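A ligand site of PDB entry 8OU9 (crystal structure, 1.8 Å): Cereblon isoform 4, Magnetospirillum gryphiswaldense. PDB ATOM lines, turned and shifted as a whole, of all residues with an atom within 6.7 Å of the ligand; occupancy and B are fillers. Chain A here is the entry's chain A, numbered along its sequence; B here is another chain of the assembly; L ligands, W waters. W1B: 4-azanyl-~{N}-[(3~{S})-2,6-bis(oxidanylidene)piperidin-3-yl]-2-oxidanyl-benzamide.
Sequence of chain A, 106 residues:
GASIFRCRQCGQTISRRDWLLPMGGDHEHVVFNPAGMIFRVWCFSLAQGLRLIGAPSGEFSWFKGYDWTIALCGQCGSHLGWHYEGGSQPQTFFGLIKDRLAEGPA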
ATOM      1  N   VAL A  31      16.888  24.240 -21.664  1.00  0.00           N
ATOM      2  CA  VAL A  31      16.631  24.005 -23.061  1.00  0.00           C
ATOM      3  C   VAL A  31      16.793  22.520 -23.282  1.00  0.00           C
ATOM      4  O   VAL A  31      17.465  21.854 -22.465  1.00  0.00           O
ATOM      5  CB  VAL A  31      17.590  24.859 -23.933  1.00  0.00           C
ATOM      6  CG1 VAL A  31      17.353  26.347 -23.714  1.00  0.00           C
ATOM      7  CG2 VAL A  31      19.022  24.548 -23.605  1.00  0.00           C
ATOM      8  N   PHE A  32      16.193  22.021 -24.351  1.00  0.00           N
ATOM      9  CA  PHE A  32      16.485  20.686 -24.839  1.00  0.00           C
ATOM     10  C   PHE A  32      16.763  20.690 -26.329  1.00  0.00           C
ATOM     11  O   PHE A  32      16.279  21.533 -27.087  1.00  0.00           O
ATOM     12  CB  PHE A  32      15.403  19.682 -24.475  1.00  0.00           C
ATOM     13  CG  PHE A  32      14.058  19.936 -25.054  1.00  0.00           C
ATOM     14  CD1 PHE A  32      13.160  20.813 -24.450  1.00  0.00           C
ATOM     15  CD2 PHE A  32      13.663  19.259 -26.210  1.00  0.00           C
ATOM     16  CE1 PHE A  32      11.901  21.012 -25.010  1.00  0.00           C
ATOM     17  CE2 PHE A  32      12.398  19.452 -26.755  1.00  0.00           C
ATOM     18  CZ  PHE A  32      11.524  20.313 -26.142  1.00  0.00           C
ATOM     19  N   ASN A  33      17.580  19.738 -26.743  1.00  0.00           N
ATOM     20  CA  ASN A  33      17.971  19.568 -28.125  1.00  0.00           C
ATOM     21  C   ASN A  33      17.089  18.471 -28.792  1.00  0.00           C
ATOM     22  O   ASN A  33      16.187  17.909 -28.181  1.00  0.00           O
ATOM     23  CB  ASN A  33      19.484  19.329 -28.150  1.00  0.00           C
ATOM     24  CG  ASN A  33      19.936  17.977 -27.636  1.00  0.00           C
ATOM     25  OD1 ASN A  33      19.104  17.116 -27.332  1.00  0.00           O
ATOM     26  ND2 ASN A  33      21.235  17.745 -27.649  1.00  0.00           N
ATOM     27  N   PRO A  34      17.294  18.207 -30.083  1.00  0.00           N
ATOM     28  CA  PRO A  34      16.511  17.195 -30.813  1.00  0.00           C
ATOM     29  C   PRO A  34      16.698  15.781 -30.278  1.00  0.00           C
ATOM     30  O   PRO A  34      15.855  14.945 -30.552  1.00  0.00           O
ATOM     31  CB  PRO A  34      17.010  17.308 -32.263  1.00  0.00           C
ATOM     32  CG  PRO A  34      17.582  18.703 -32.393  1.00  0.00           C
ATOM     33  CD  PRO A  34      18.162  18.993 -31.017  1.00  0.00           C
ATOM     34  N   ALA A  35      17.794  15.513 -29.524  1.00  0.00           N
ATOM     35  CA  ALA A  35      18.010  14.234 -28.915  1.00  0.00           C
ATOM     36  C   ALA A  35      17.387  14.157 -27.530  1.00  0.00           C
ATOM     37  O   ALA A  35      17.704  13.223 -26.799  1.00  0.00           O
ATOM     38  CB  ALA A  35      19.415  13.816 -28.885  1.00  0.00           C
ATOM     39  N   MET A  37      18.072  15.793 -24.889  1.00  0.00           N
ATOM     40  CA  MET A  37      18.915  16.131 -23.755  1.00  0.00           C
ATOM     41  C   MET A  37      18.536  17.511 -23.238  1.00  0.00           C
ATOM     42  O   MET A  37      18.405  18.461 -24.024  1.00  0.00           O
ATOM     43  CB  MET A  37      20.386  16.127 -24.168  1.00  0.00           C
ATOM     44  CG  MET A  37      20.773  14.971 -25.044  1.00  0.00           C
ATOM     45  SD  MET A  37      22.469  15.115 -25.688  1.00  0.00           S
ATOM     46  N   PHE A  39      19.540  20.752 -20.926  1.00  0.00           N
ATOM     47  CA  PHE A  39      20.719  21.477 -20.469  1.00  0.00           C
ATOM     48  C   PHE A  39      20.286  22.663 -19.671  1.00  0.00           C
ATOM     49  O   PHE A  39      19.343  23.395 -20.114  1.00  0.00           O
ATOM     50  CB  PHE A  39      21.548  22.009 -21.656  1.00  0.00           C
ATOM     51  CG  PHE A  39      22.094  20.955 -22.571  1.00  0.00           C
ATOM     52  CD1 PHE A  39      23.192  20.198 -22.222  1.00  0.00           C
ATOM     53  CD2 PHE A  39      21.390  20.613 -23.719  1.00  0.00           C
ATOM     54  CE1 PHE A  39      23.646  19.233 -23.106  1.00  0.00           C
ATOM     55  CE2 PHE A  39      21.898  19.671 -24.613  1.00  0.00           C
ATOM     56  CZ  PHE A  39      23.007  18.966 -24.306  1.00  0.00           C
ATOM     57  N   GLU A  59      20.324  26.018 -37.278  1.00  0.00           N
ATOM     58  CA  GLU A  59      19.368  24.954 -37.012  1.00  0.00           C
ATOM     59  C   GLU A  59      19.101  24.766 -35.515  1.00  0.00           C
ATOM     60  O   GLU A  59      20.016  24.535 -34.757  1.00  0.00           O
ATOM     61  CB  GLU A  59      19.906  23.611 -37.522  1.00  0.00           C
ATOM     62  CG  GLU A  59      20.404  23.601 -38.946  1.00  0.00           C
ATOM     63  N   PHE A  60      17.837  24.794 -35.088  1.00  0.00           N
ATOM     64  CA  PHE A  60      17.459  24.457 -33.708  1.00  0.00           C
ATOM     65  C   PHE A  60      18.009  25.462 -32.697  1.00  0.00           C
ATOM     66  O   PHE A  60      17.985  25.256 -31.488  1.00  0.00           O
ATOM     67  CB  PHE A  60      17.890  23.044 -33.369  1.00  0.00           C
ATOM     68  CG  PHE A  60      17.433  21.951 -34.306  1.00  0.00           C
ATOM     69  CD1 PHE A  60      16.090  21.649 -34.412  1.00  0.00           C
ATOM     70  CD2 PHE A  60      18.344  21.167 -34.955  1.00  0.00           C
ATOM     71  CE1 PHE A  60      15.659  20.582 -35.179  1.00  0.00           C
ATOM     72  CE2 PHE A  60      17.936  20.117 -35.759  1.00  0.00           C
ATOM     73  CZ  PHE A  60      16.577  19.822 -35.855  1.00  0.00           C
ATOM     74  N   SER A  61      18.479  26.629 -33.161  1.00  0.00           N
ATOM     75  CA  SER A  61      19.008  27.581 -32.229  1.00  0.00           C
ATOM     76  C   SER A  61      17.993  27.968 -31.174  1.00  0.00           C
ATOM     77  O   SER A  61      16.881  28.376 -31.475  1.00  0.00           O
ATOM     78  CB  SER A  61      19.668  28.779 -32.878  1.00  0.00           C
ATOM     79  OG  SER A  61      20.018  29.719 -31.862  1.00  0.00           O
ATOM     80  N   TRP A  62      18.434  27.881 -29.920  1.00  0.00           N
ATOM     81  CA  TRP A  62      17.631  28.258 -28.794  1.00  0.00           C
ATOM     82  C   TRP A  62      17.465  29.753 -28.688  1.00  0.00           C
ATOM     83  O   TRP A  62      16.725  30.239 -27.871  1.00  0.00           O
ATOM     84  CB  TRP A  62      18.187  27.720 -27.476  1.00  0.00           C
ATOM     85  CG  TRP A  62      18.155  26.244 -27.427  1.00  0.00           C
ATOM     86  CD1 TRP A  62      17.097  25.409 -27.664  1.00  0.00           C
ATOM     87  CD2 TRP A  62      19.235  25.412 -27.055  1.00  0.00           C
ATOM     88  NE1 TRP A  62      17.481  24.106 -27.484  1.00  0.00           N
ATOM     89  CE2 TRP A  62      18.780  24.079 -27.067  1.00  0.00           C
ATOM     90  CE3 TRP A  62      20.578  25.669 -26.749  1.00  0.00           C
ATOM     91  CZ2 TRP A  62      19.624  23.012 -26.853  1.00  0.00           C
ATOM     92  CZ3 TRP A  62      21.384  24.617 -26.465  1.00  0.00           C
ATOM     93  CH2 TRP A  62      20.915  23.282 -26.457  1.00  0.00           C
ATOM     94  N   PHE A  63      18.328  30.507 -29.361  1.00  0.00           N
ATOM     95  CA  PHE A  63      18.356  31.930 -29.149  1.00  0.00           C
ATOM     96  C   PHE A  63      18.101  32.602 -30.499  1.00  0.00           C
ATOM     97  O   PHE A  63      18.846  32.455 -31.476  1.00  0.00           O
ATOM     98  CB  PHE A  63      19.726  32.371 -28.582  1.00  0.00           C
ATOM     99  CG  PHE A  63      20.019  31.829 -27.221  1.00  0.00           C
ATOM    100  CD1 PHE A  63      19.457  32.409 -26.092  1.00  0.00           C
ATOM    101  CD2 PHE A  63      20.788  30.699 -27.066  1.00  0.00           C
ATOM    102  CE1 PHE A  63      19.774  31.968 -24.828  1.00  0.00           C
ATOM    103  CE2 PHE A  63      21.023  30.191 -25.787  1.00  0.00           C
ATOM    104  CZ  PHE A  63      20.518  30.848 -24.658  1.00  0.00           C
ATOM    105  N   TYR A  66      20.567  33.939 -33.637  1.00  0.00           N
ATOM    106  CA  TYR A  66      21.950  33.530 -33.442  1.00  0.00           C
ATOM    107  C   TYR A  66      22.143  32.181 -34.045  1.00  0.00           C
ATOM    108  O   TYR A  66      21.270  31.292 -33.997  1.00  0.00           O
ATOM    109  CB  TYR A  66      22.323  33.452 -31.936  1.00  0.00           C
ATOM    110  CG  TYR A  66      22.257  34.734 -31.198  1.00  0.00           C
ATOM    111  CD1 TYR A  66      23.321  35.613 -31.210  1.00  0.00           C
ATOM    112  CD2 TYR A  66      21.085  35.157 -30.574  1.00  0.00           C
ATOM    113  CE1 TYR A  66      23.316  36.800 -30.531  1.00  0.00           C
ATOM    114  CE2 TYR A  66      21.042  36.392 -29.931  1.00  0.00           C
ATOM    115  CZ  TYR A  66      22.129  37.235 -29.980  1.00  0.00           C
ATOM    116  OH  TYR A  66      22.160  38.384 -29.276  1.00  0.00           O
ATOM    117  N   TRP A  68      25.004  28.957 -33.940  1.00  0.00           N
ATOM    118  CA  TRP A  68      25.853  28.379 -32.893  1.00  0.00           C
ATOM    119  C   TRP A  68      26.997  27.580 -33.518  1.00  0.00           C
ATOM    120  O   TRP A  68      26.846  26.971 -34.589  1.00  0.00           O
ATOM    121  CB  TRP A  68      25.015  27.511 -31.953  1.00  0.00           C
ATOM    122  CG  TRP A  68      24.168  26.501 -32.667  1.00  0.00           C
ATOM    123  CD1 TRP A  68      22.831  26.608 -32.957  1.00  0.00           C
ATOM    124  CD2 TRP A  68      24.565  25.171 -33.068  1.00  0.00           C
ATOM    125  NE1 TRP A  68      22.439  25.506 -33.677  1.00  0.00           N
ATOM    126  CE2 TRP A  68      23.458  24.597 -33.723  1.00  0.00           C
ATOM    127  CE3 TRP A  68      25.773  24.465 -33.031  1.00  0.00           C
ATOM    128  CZ2 TRP A  68      23.505  23.346 -34.286  1.00  0.00           C
ATOM    129  CZ3 TRP A  68      25.814  23.195 -33.591  1.00  0.00           C
ATOM    130  CH2 TRP A  68      24.660  22.622 -34.159  1.00  0.00           C
ATOM    131  N   ILE A  70      29.662  24.591 -31.672  1.00  0.00           N
ATOM    132  CA  ILE A  70      30.019  23.772 -30.522  1.00  0.00           C
ATOM    133  C   ILE A  70      31.301  24.291 -29.867  1.00  0.00           C
ATOM    134  O   ILE A  70      32.290  24.599 -30.541  1.00  0.00           O
ATOM    135  CB  ILE A  70      30.182  22.324 -30.978  1.00  0.00           C
ATOM    136  CG1 ILE A  70      28.821  21.794 -31.444  1.00  0.00           C
ATOM    137  CG2 ILE A  70      30.698  21.483 -29.795  1.00  0.00           C
ATOM    138  CD1 ILE A  70      28.906  20.533 -32.311  1.00  0.00           C
ATOM    139  N   HIS A  79      32.605  18.622 -23.994  1.00  0.00           N
ATOM    140  CA  HIS A  79      31.635  19.570 -24.516  1.00  0.00           C
ATOM    141  C   HIS A  79      31.139  20.491 -23.443  1.00  0.00           C
ATOM    142  O   HIS A  79      30.488  20.036 -22.493  1.00  0.00           O
ATOM    143  CB  HIS A  79      30.490  18.776 -25.157  1.00  0.00           C
ATOM    144  CG  HIS A  79      29.491  19.688 -25.744  1.00  0.00           C
ATOM    145  ND1 HIS A  79      28.140  19.377 -25.751  1.00  0.00           N
ATOM    146  CD2 HIS A  79      29.599  20.949 -26.257  1.00  0.00           C
ATOM    147  CE1 HIS A  79      27.478  20.372 -26.356  1.00  0.00           C
ATOM    148  NE2 HIS A  79      28.315  21.324 -26.676  1.00  0.00           N
ATOM    149  N   TRP A  82      28.200  26.163 -26.231  1.00  0.00           N
ATOM    150  CA  TRP A  82      28.113  26.702 -27.600  1.00  0.00           C
ATOM    151  C   TRP A  82      28.491  28.150 -27.613  1.00  0.00           C
ATOM    152  O   TRP A  82      28.270  28.864 -26.657  1.00  0.00           O
ATOM    153  CB  TRP A  82      26.678  26.518 -28.213  1.00  0.00           C
ATOM    154  CG  TRP A  82      26.147  25.111 -28.132  1.00  0.00           C
ATOM    155  CD1 TRP A  82      26.194  24.183 -29.097  1.00  0.00           C
ATOM    156  CD2 TRP A  82      25.540  24.444 -26.995  1.00  0.00           C
ATOM    157  NE1 TRP A  82      25.730  22.975 -28.613  1.00  0.00           N
ATOM    158  CE2 TRP A  82      25.261  23.144 -27.360  1.00  0.00           C
ATOM    159  CE3 TRP A  82      25.175  24.896 -25.715  1.00  0.00           C
ATOM    160  CZ2 TRP A  82      24.651  22.246 -26.476  1.00  0.00           C
ATOM    161  CZ3 TRP A  82      24.615  24.012 -24.839  1.00  0.00           C
ATOM    162  CH2 TRP A  82      24.353  22.723 -25.225  1.00  0.00           C
ATOM    163  N   TYR A  84      27.641  31.575 -29.641  1.00  0.00           N
ATOM    164  CA  TYR A  84      26.553  32.094 -30.461  1.00  0.00           C
ATOM    165  C   TYR A  84      27.042  33.386 -31.171  1.00  0.00           C
ATOM    166  O   TYR A  84      27.679  34.181 -30.526  1.00  0.00           O
ATOM    167  CB  TYR A  84      25.363  32.449 -29.568  1.00  0.00           C
ATOM    168  CG  TYR A  84      24.631  31.209 -29.133  1.00  0.00           C
ATOM    169  CD1 TYR A  84      23.726  30.571 -29.945  1.00  0.00           C
ATOM    170  CD2 TYR A  84      25.006  30.584 -27.950  1.00  0.00           C
ATOM    171  CE1 TYR A  84      23.099  29.397 -29.551  1.00  0.00           C
ATOM    172  CE2 TYR A  84      24.349  29.427 -27.514  1.00  0.00           C
ATOM    173  CZ  TYR A  84      23.463  28.792 -28.337  1.00  0.00           C
ATOM    174  OH  TYR A  84      22.855  27.555 -27.907  1.00  0.00           O
ATOM    175  N   PRO B 105      13.046  22.049 -29.834  1.00  0.00           N
ATOM    176  CA  PRO B 105      12.429  21.734 -31.129  1.00  0.00           C
ATOM    177  C   PRO B 105      11.339  20.673 -31.110  1.00  0.00           C
ATOM    178  O   PRO B 105      11.280  19.843 -30.187  1.00  0.00           O
ATOM    179  CB  PRO B 105      13.596  21.172 -31.970  1.00  0.00           C
ATOM    180  CG  PRO B 105      14.626  20.702 -30.951  1.00  0.00           C
ATOM    181  CD  PRO B 105      14.478  21.651 -29.774  1.00  0.00           C
HETATM  182  C4  W1B L   1      21.354  25.151 -29.974  1.00  0.00           C
HETATM  183  C5  W1B L   1      20.434  22.908 -30.138  1.00  0.00           C
HETATM  184  C6  W1B L   1      22.137  19.960 -30.480  1.00  0.00           C
HETATM  185  N1  W1B L   1      20.337  24.253 -30.036  1.00  0.00           N
HETATM  186  N3  W1B L   1      21.226  15.368 -33.662  1.00  0.00           N
HETATM  187  C2  W1B L   1      22.903  23.237 -30.563  1.00  0.00           C
HETATM  188  C1  W1B L   1      21.804  22.293 -30.084  1.00  0.00           C
HETATM  189  C3  W1B L   1      22.700  24.567 -29.859  1.00  0.00           C
HETATM  190  O1  W1B L   1      19.424  22.243 -30.254  1.00  0.00           O
HETATM  191  O2  W1B L   1      21.100  26.313 -29.752  1.00  0.00           O
HETATM  192  N2  W1B L   1      21.815  21.151 -30.954  1.00  0.00           N
HETATM  193  C7  W1B L   1      21.920  18.835 -31.411  1.00  0.00           C
HETATM  194  O3  W1B L   1      22.519  19.790 -29.306  1.00  0.00           O
HETATM  195  C8  W1B L   1      22.057  17.568 -30.859  1.00  0.00           C
HETATM  196  C9  W1B L   1      21.835  16.442 -31.588  1.00  0.00           C
HETATM  197  C10 W1B L   1      21.428  16.532 -32.933  1.00  0.00           C
HETATM  198  C11 W1B L   1      21.275  17.812 -33.499  1.00  0.00           C
HETATM  199  C12 W1B L   1      21.534  18.949 -32.757  1.00  0.00           C
HETATM  200  O4  W1B L   1      21.367  20.169 -33.325  1.00  0.00           O
HETATM  201  O   HOH W   1      21.769  20.689 -36.125  1.00  0.00           O
HETATM  202  O   HOH W   2      25.461  20.437 -29.531  1.00  0.00           O
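The side-chain hydroxyl (OH) of Tyr 84 lies within hydrogen-bond range of an oxygen (O2) of the ligand (2.8 Å). The side-chain amide nitrogen (ND2) of Asn 33 lies within hydrogen-bond range of an oxygen (O3) of the ligand. A nitrogen (N1) of the ligand lies within hydrogen-bond range of the backbone carbonyl oxygen (O) of Phe 60. The backbone NH (N) of Trp 62 is in hydrogen-bond range of an oxygen (O2) of the ligand, 3.1 Å away.
The backbone NH (N) of Ala 35 lies within hydrogen-bond range of the side-chain amide oxygen (OD1) of Asn 33 (3.0 Å). N of Met 37 is in hydrogen-bond range of OD1 of Asn 33, at 3.0 Å. The backbone carbonyl oxygen (O) of Phe 32 is in hydrogen-bond range of the indole nitrogen (NE1) of Trp 62 (2.9 Å). The side-chain hydroxyl (OG) of Ser 61 sits at hydrogen-bond distance from the backbone carbonyl oxygen (O) of Phe 63 (3.0 Å). The backbone carbonyl oxygen of Tyr 66 is in hydrogen-bond range of the side-chain hydroxyl of Ser 61. NE1 of Trp 68 sits at hydrogen-bond distance from O of Glu 59 (2.8 Å).
CD of Pro 34 touches O1 of the ligand (3.6 Å). Ser 61 touches the ligand. CE2 of Trp 68 touches C2 of the ligand, 3.5 Å away. Trp 82 touches the ligand. Hydrophobic or aromatic side chains within 4 Å of the ligand: Pro 34, Phe 60, Trp 62, Trp 68, Trp 82 and Tyr 84. Of the 19 residues printed, 8 come within 4 Å of the ligand. The nearest printed residue that does not touch the ligand is Ala 35 (4.5 Å).
Water W2 lies within hydrogen-bond range of NE1 of Trp 82 (2.7 Å) and O3 of the ligand (3.0 Å).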
